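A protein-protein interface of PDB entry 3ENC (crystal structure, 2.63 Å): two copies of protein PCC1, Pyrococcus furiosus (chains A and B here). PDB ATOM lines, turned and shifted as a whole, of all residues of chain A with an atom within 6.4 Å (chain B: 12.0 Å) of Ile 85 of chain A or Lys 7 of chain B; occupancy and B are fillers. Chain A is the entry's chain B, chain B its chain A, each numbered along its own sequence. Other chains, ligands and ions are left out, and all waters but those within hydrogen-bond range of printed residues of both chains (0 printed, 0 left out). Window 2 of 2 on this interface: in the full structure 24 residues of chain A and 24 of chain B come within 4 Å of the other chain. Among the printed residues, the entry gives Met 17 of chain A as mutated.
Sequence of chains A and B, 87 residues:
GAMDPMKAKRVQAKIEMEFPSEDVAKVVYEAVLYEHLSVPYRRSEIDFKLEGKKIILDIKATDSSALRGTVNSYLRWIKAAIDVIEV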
ATOM      1  N   MET A  17      37.218  -4.547  24.952  1.00  0.00           N
ATOM      2  CA  MET A  17      35.758  -4.378  25.004  1.00  0.00           C
ATOM      3  C   MET A  17      35.090  -4.392  23.611  1.00  0.00           C
ATOM      4  O   MET A  17      35.494  -3.632  22.730  1.00  0.00           O
ATOM      5  CB  MET A  17      35.381  -3.087  25.748  1.00  0.00           C
ATOM      6  CG  MET A  17      35.000  -3.281  27.209  1.00  0.00           C
ATOM      7  SD  MET A  17      33.365  -2.321  27.738  1.00  0.00           S
ATOM      8  CE  MET A  17      32.117  -3.059  26.427  1.00  0.00           C
ATOM      9  N   GLU A  18      34.067  -5.235  23.426  1.00  0.00           N
ATOM     10  CA  GLU A  18      33.350  -5.343  22.146  1.00  0.00           C
ATOM     11  C   GLU A  18      32.012  -4.620  22.245  1.00  0.00           C
ATOM     12  O   GLU A  18      31.310  -4.720  23.252  1.00  0.00           O
ATOM     13  CB  GLU A  18      33.145  -6.811  21.750  1.00  0.00           C
ATOM     14  CG  GLU A  18      33.013  -7.073  20.240  1.00  0.00           C
ATOM     15  CD  GLU A  18      34.221  -7.792  19.639  1.00  0.00           C
ATOM     16  OE1 GLU A  18      35.113  -8.213  20.406  1.00  0.00           O
ATOM     17  OE2 GLU A  18      34.274  -7.947  18.397  1.00  0.00           O
ATOM     18  N   PHE A  19      31.654  -3.892  21.198  1.00  0.00           N
ATOM     19  CA  PHE A  19      30.535  -2.971  21.307  1.00  0.00           C
ATOM     20  C   PHE A  19      29.448  -3.169  20.275  1.00  0.00           C
ATOM     21  O   PHE A  19      29.680  -3.777  19.227  1.00  0.00           O
ATOM     22  CB  PHE A  19      31.033  -1.528  21.238  1.00  0.00           C
ATOM     23  CG  PHE A  19      31.304  -0.916  22.579  1.00  0.00           C
ATOM     24  CD1 PHE A  19      30.283  -0.317  23.306  1.00  0.00           C
ATOM     25  CD2 PHE A  19      32.579  -0.929  23.112  1.00  0.00           C
ATOM     26  CE1 PHE A  19      30.533   0.250  24.537  1.00  0.00           C
ATOM     27  CE2 PHE A  19      32.833  -0.361  24.344  1.00  0.00           C
ATOM     28  CZ  PHE A  19      31.807   0.230  25.056  1.00  0.00           C
ATOM     29  N   PRO A  20      28.251  -2.635  20.571  1.00  0.00           N
ATOM     30  CA  PRO A  20      27.167  -2.572  19.591  1.00  0.00           C
ATOM     31  C   PRO A  20      27.709  -2.170  18.200  1.00  0.00           C
ATOM     32  O   PRO A  20      28.066  -3.069  17.441  1.00  0.00           O
ATOM     33  CB  PRO A  20      26.233  -1.511  20.185  1.00  0.00           C
ATOM     34  CG  PRO A  20      26.416  -1.669  21.674  1.00  0.00           C
ATOM     35  CD  PRO A  20      27.868  -2.034  21.867  1.00  0.00           C
ATOM     36  N   VAL A  24      29.593   3.139  17.486  1.00  0.00           N
ATOM     37  CA  VAL A  24      29.156   3.467  18.853  1.00  0.00           C
ATOM     38  C   VAL A  24      30.352   3.364  19.796  1.00  0.00           C
ATOM     39  O   VAL A  24      30.421   4.041  20.822  1.00  0.00           O
ATOM     40  CB  VAL A  24      28.023   2.528  19.364  1.00  0.00           C
ATOM     41  CG1 VAL A  24      28.006   2.462  20.895  1.00  0.00           C
ATOM     42  CG2 VAL A  24      26.672   2.979  18.841  1.00  0.00           C
ATOM     43  N   VAL A  27      32.614   6.501  19.470  1.00  0.00           N
ATOM     44  CA  VAL A  27      32.238   7.608  20.343  1.00  0.00           C
ATOM     45  C   VAL A  27      32.909   7.509  21.701  1.00  0.00           C
ATOM     46  O   VAL A  27      33.405   8.508  22.233  1.00  0.00           O
ATOM     47  CB  VAL A  27      30.741   7.647  20.576  1.00  0.00           C
ATOM     48  CG1 VAL A  27      30.412   8.601  21.712  1.00  0.00           C
ATOM     49  CG2 VAL A  27      30.044   8.057  19.312  1.00  0.00           C
ATOM     50  N   VAL A  28      32.905   6.301  22.263  1.00  0.00           N
ATOM     51  CA  VAL A  28      33.521   6.058  23.561  1.00  0.00           C
ATOM     52  C   VAL A  28      35.014   6.335  23.522  1.00  0.00           C
ATOM     53  O   VAL A  28      35.518   7.125  24.324  1.00  0.00           O
ATOM     54  CB  VAL A  28      33.257   4.628  24.060  1.00  0.00           C
ATOM     55  CG1 VAL A  28      34.456   4.100  24.851  1.00  0.00           C
ATOM     56  CG2 VAL A  28      31.984   4.586  24.893  1.00  0.00           C
ATOM     57  N   ALA A  81      31.361   7.610  29.388  1.00  0.00           N
ATOM     58  CA  ALA A  81      31.098   7.728  27.967  1.00  0.00           C
ATOM     59  C   ALA A  81      29.829   6.949  27.594  1.00  0.00           C
ATOM     60  O   ALA A  81      28.967   7.466  26.882  1.00  0.00           O
ATOM     61  CB  ALA A  81      32.299   7.223  27.179  1.00  0.00           C
ATOM     62  N   ILE A  82      29.720   5.715  28.086  1.00  0.00           N
ATOM     63  CA  ILE A  82      28.553   4.861  27.847  1.00  0.00           C
ATOM     64  C   ILE A  82      27.211   5.575  28.123  1.00  0.00           C
ATOM     65  O   ILE A  82      26.248   5.424  27.361  1.00  0.00           O
ATOM     66  CB  ILE A  82      28.662   3.516  28.650  1.00  0.00           C
ATOM     67  CG1 ILE A  82      29.773   2.639  28.083  1.00  0.00           C
ATOM     68  CG2 ILE A  82      27.351   2.732  28.639  1.00  0.00           C
ATOM     69  CD1 ILE A  82      29.592   2.349  26.630  1.00  0.00           C
ATOM     70  N   ASP A  83      27.160   6.378  29.185  1.00  0.00           N
ATOM     71  CA  ASP A  83      25.898   6.983  29.626  1.00  0.00           C
ATOM     72  C   ASP A  83      25.513   8.320  28.944  1.00  0.00           C
ATOM     73  O   ASP A  83      24.497   8.930  29.284  1.00  0.00           O
ATOM     74  CB  ASP A  83      25.853   7.070  31.164  1.00  0.00           C
ATOM     75  CG  ASP A  83      25.647   5.698  31.825  1.00  0.00           C
ATOM     76  OD1 ASP A  83      24.841   4.891  31.304  1.00  0.00           O
ATOM     77  OD2 ASP A  83      26.286   5.423  32.864  1.00  0.00           O
ATOM     78  N   VAL A  84      26.312   8.751  27.970  1.00  0.00           N
ATOM     79  CA  VAL A  84      25.954   9.871  27.102  1.00  0.00           C
ATOM     80  C   VAL A  84      25.679   9.359  25.681  1.00  0.00           C
ATOM     81  O   VAL A  84      26.346   9.759  24.724  1.00  0.00           O
ATOM     82  CB  VAL A  84      27.069  10.934  27.029  1.00  0.00           C
ATOM     83  CG1 VAL A  84      26.520  12.213  26.410  1.00  0.00           C
ATOM     84  CG2 VAL A  84      27.631  11.227  28.402  1.00  0.00           C
ATOM     85  N   ILE A  85      24.698   8.470  25.547  1.00  0.00           N
ATOM     86  CA  ILE A  85      24.400   7.842  24.261  1.00  0.00           C
ATOM     87  C   ILE A  85      22.902   7.581  24.060  1.00  0.00           C
ATOM     88  O   ILE A  85      22.271   6.838  24.819  1.00  0.00           O
ATOM     89  CB  ILE A  85      25.193   6.521  24.086  1.00  0.00           C
ATOM     90  CG1 ILE A  85      26.701   6.800  24.018  1.00  0.00           C
ATOM     91  CG2 ILE A  85      24.719   5.760  22.842  1.00  0.00           C
ATOM     92  CD1 ILE A  85      27.531   5.553  23.857  1.00  0.00           C
ATOM     93  N   LYS B   7      25.148  -0.040  28.082  1.00  0.00           N
ATOM     94  CA  LYS B   7      25.046  -0.644  26.763  1.00  0.00           C
ATOM     95  C   LYS B   7      26.419  -1.185  26.357  1.00  0.00           C
ATOM     96  O   LYS B   7      26.890  -0.968  25.230  1.00  0.00           O
ATOM     97  CB  LYS B   7      24.511   0.370  25.752  1.00  0.00           C
ATOM     98  CG  LYS B   7      23.361  -0.149  24.890  1.00  0.00           C
ATOM     99  CD  LYS B   7      22.763   0.955  24.037  1.00  0.00           C
ATOM    100  CE  LYS B   7      23.739   1.432  22.955  1.00  0.00           C
ATOM    101  NZ  LYS B   7      24.931   2.142  23.501  1.00  0.00           N
ATOM    102  N   ALA B   8      27.051  -1.885  27.302  1.00  0.00           N
ATOM    103  CA  ALA B   8      28.348  -2.530  27.092  1.00  0.00           C
ATOM    104  C   ALA B   8      28.161  -4.047  27.017  1.00  0.00           C
ATOM    105  O   ALA B   8      27.382  -4.623  27.789  1.00  0.00           O
ATOM    106  CB  ALA B   8      29.295  -2.174  28.215  1.00  0.00           C
ATOM    107  N   LYS B   9      28.902  -4.694  26.117  1.00  0.00           N
ATOM    108  CA  LYS B   9      28.637  -6.093  25.748  1.00  0.00           C
ATOM    109  C   LYS B   9      29.532  -7.161  26.408  1.00  0.00           C
ATOM    110  O   LYS B   9      29.426  -7.384  27.618  1.00  0.00           O
ATOM    111  CB  LYS B   9      28.616  -6.238  24.222  1.00  0.00           C
ATOM    112  CG  LYS B   9      27.207  -6.285  23.639  1.00  0.00           C
ATOM    113  CD  LYS B   9      26.187  -5.438  24.412  1.00  0.00           C
ATOM    114  CE  LYS B   9      26.335  -3.946  24.136  1.00  0.00           C
ATOM    115  NZ  LYS B   9      25.132  -3.149  24.549  1.00  0.00           N
ATOM    116  N   ARG B  10      30.377  -7.847  25.633  1.00  0.00           N
ATOM    117  CA  ARG B  10      31.281  -8.851  26.225  1.00  0.00           C
ATOM    118  C   ARG B  10      32.647  -8.257  26.588  1.00  0.00           C
ATOM    119  O   ARG B  10      33.284  -7.611  25.757  1.00  0.00           O
ATOM    120  CB  ARG B  10      31.451 -10.074  25.320  1.00  0.00           C
ATOM    121  CG  ARG B  10      32.879 -10.336  24.839  1.00  0.00           C
ATOM    122  CD  ARG B  10      33.034 -10.076  23.349  1.00  0.00           C
ATOM    123  NE  ARG B  10      34.403 -10.323  22.898  1.00  0.00           N
ATOM    124  CZ  ARG B  10      34.773 -11.338  22.121  1.00  0.00           C
ATOM    125  NH1 ARG B  10      36.046 -11.476  21.769  1.00  0.00           N
ATOM    126  NH2 ARG B  10      33.875 -12.210  21.682  1.00  0.00           N
ATOM    127  N   VAL B  11      33.099  -8.484  27.820  1.00  0.00           N
ATOM    128  CA  VAL B  11      34.290  -7.804  28.322  1.00  0.00           C
ATOM    129  C   VAL B  11      35.299  -8.736  29.001  1.00  0.00           C
ATOM    130  O   VAL B  11      34.928  -9.522  29.873  1.00  0.00           O
ATOM    131  CB  VAL B  11      33.895  -6.647  29.269  1.00  0.00           C
ATOM    132  CG1 VAL B  11      33.035  -5.653  28.530  1.00  0.00           C
ATOM    133  CG2 VAL B  11      33.141  -7.159  30.470  1.00  0.00           C
ATOM    134  N   ALA B  61      33.367 -10.226  32.398  1.00  0.00           N
ATOM    135  CA  ALA B  61      32.254  -9.534  33.041  1.00  0.00           C
ATOM    136  C   ALA B  61      31.057  -9.385  32.114  1.00  0.00           C
ATOM    137  O   ALA B  61      31.213  -9.080  30.930  1.00  0.00           O
ATOM    138  CB  ALA B  61      32.697  -8.177  33.538  1.00  0.00           C
ATOM    139  N   THR B  62      29.859  -9.599  32.652  1.00  0.00           N
ATOM    140  CA  THR B  62      28.667  -9.350  31.863  1.00  0.00           C
ATOM    141  C   THR B  62      28.822  -7.944  31.281  1.00  0.00           C
ATOM    142  O   THR B  62      28.428  -7.682  30.148  1.00  0.00           O
ATOM    143  CB  THR B  62      27.345  -9.516  32.677  1.00  0.00           C
ATOM    144  OG1 THR B  62      27.116  -8.367  33.499  1.00  0.00           O
ATOM    145  CG2 THR B  62      27.397 -10.759  33.558  1.00  0.00           C
ATOM    146  N   ASP B  63      29.446  -7.050  32.037  1.00  0.00           N
ATOM    147  CA  ASP B  63      29.596  -5.687  31.561  1.00  0.00           C
ATOM    148  C   ASP B  63      30.729  -4.885  32.193  1.00  0.00           C
ATOM    149  O   ASP B  63      31.574  -5.407  32.921  1.00  0.00           O
ATOM    150  CB  ASP B  63      28.285  -4.932  31.742  1.00  0.00           C
ATOM    151  CG  ASP B  63      27.910  -4.769  33.199  1.00  0.00           C
ATOM    152  OD1 ASP B  63      28.726  -5.143  34.063  1.00  0.00           O
ATOM    153  OD2 ASP B  63      26.803  -4.266  33.482  1.00  0.00           O
ATOM    154  N   SER B  64      30.697  -3.589  31.907  1.00  0.00           N
ATOM    155  CA  SER B  64      31.805  -2.667  32.161  1.00  0.00           C
ATOM    156  C   SER B  64      32.177  -2.604  33.619  1.00  0.00           C
ATOM    157  O   SER B  64      33.317  -2.344  33.973  1.00  0.00           O
ATOM    158  CB  SER B  64      31.463  -1.260  31.638  1.00  0.00           C
ATOM    159  OG  SER B  64      30.061  -1.071  31.508  1.00  0.00           O
ATOM    160  N   SER B  65      31.202  -2.858  34.473  1.00  0.00           N
ATOM    161  CA  SER B  65      31.427  -2.754  35.900  1.00  0.00           C
ATOM    162  C   SER B  65      31.328  -4.106  36.566  1.00  0.00           C
ATOM    163  O   SER B  65      31.817  -4.283  37.681  1.00  0.00           O
ATOM    164  CB  SER B  65      30.447  -1.765  36.522  1.00  0.00           C
ATOM    165  OG  SER B  65      30.763  -0.449  36.111  1.00  0.00           O
ATOM    166  N   ALA B  66      30.716  -5.069  35.885  1.00  0.00           N
ATOM    167  CA  ALA B  66      30.706  -6.431  36.398  1.00  0.00           C
ATOM    168  C   ALA B  66      32.165  -6.836  36.570  1.00  0.00           C
ATOM    169  O   ALA B  66      32.486  -7.889  37.144  1.00  0.00           O
ATOM    170  CB  ALA B  66      29.986  -7.367  35.440  1.00  0.00           C
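No position is printed for both chains.
Of chain B, only Lys 7 comes within 4 Å of Ile 85 of chain A. Of chain A, only Phe 19, Pro 20, Ile 82 and Ile 85 come within 4 Å of Lys 7 of chain B. Phe 19 of chain A touches just one residue of chain B: Lys 7 (3.9 Å). No residue of chain B comes within 4 Å of Val 24 of chain A. No residue of chain B comes within 4 Å of Val 27 of chain A. No residue of chain B comes within 4 Å of Ala 81 of chain A. Of chain B, only Lys 7 (3.6 Å) comes within 4 Å of Ile 82 of chain A. No residue of chain B comes within 4 Å of Val 84 of chain A. Of the printed residues of chain B, Met 17 of chain A touches Ala 8 (3.5 Å), Lys 9 (3.6 Å) and Val 11 (3.4 Å). Printed residues of chain A within 4 Å of Lys 9 of chain B: Met 17 (3.6 Å), Glu 18 (3.2 Å) and Pro 20 (3.3 Å). Of the printed residues of chain B, Pro 20 of chain A touches Lys 7 and Lys 9. Of the printed residues of chain A, Val 11 of chain B touches Met 17 (3.4 Å). Of the printed residues of chain A, Ala 8 of chain B touches Met 17. Ser 65 of chain B touches none of the printed residues of chain A. Ala 66 of chain B touches none of the printed residues of chain A. The nearest printed residue of chain A that does not touch Arg 10 of chain B is Met 17 of chain A (4.1 Å).
Of the 11 printed residues of chain B, 5 touch a printed residue of chain A. Printed residues of chain B that touch a printed residue of chain A: Lys 7, Ala 8, Lys 9, Arg 10 and Val 11. Hydrophobic or aromatic side chains of chain B that line the printed part of chain A: Ala 8 and Val 11. Of the 12 printed residues of chain A, 6 touch a printed residue of chain B. Hydrophobic or aromatic side chains of chain A that line the printed part of chain B: Met 17, Phe 19, Pro 20, Ile 82 and Ile 85. Among the printed residues, 10 pairs touch across the chains. Among the printed residues, Asp or Glu carboxylates within 4 Å of a Lys or Arg side-chain nitrogen of the other chain: Glu 18 of chain A with Arg 10 of chain B (3.3 Å).
NE of Arg 10 of chain B lies within salt-bridge range of OE1 of Glu 18 of chain A, at 3.3 Å.
The backbone carbonyl oxygen (O) of Lys 7 of chain B is in hydrogen-bond range of the side-chain amino group (NZ) of Lys 9 of chain B (2.9 Å). O of Thr 62 of chain B sits close to O of Lys 9 of chain B. O of Val 11 of chain B sits at hydrogen-bond distance from N of Ala 61 of chain B (3.1 Å).
Among the printed residues, pairs that only touch across the chains: Met 17 of chain A with Ala 8 of chain B (3.5 Å), Met 17 of chain A with Lys 9 of chain B (3.6 Å), Met 17 of chain A with Val 11 of chain B (3.4 Å), Glu 18 of chain A with Lys 9 of chain B (3.2 Å), Phe 19 of chain A with Lys 7 of chain B (3.9 Å), Pro 20 of chain A with Lys 7 of chain B (3.7 Å), Pro 20 of chain A with Lys 9 of chain B (3.3 Å), Ile 82 of chain A with Lys 7 of chain B (3.6 Å) and Ile 85 of chain A with Lys 7 of chain B (3.7 Å).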
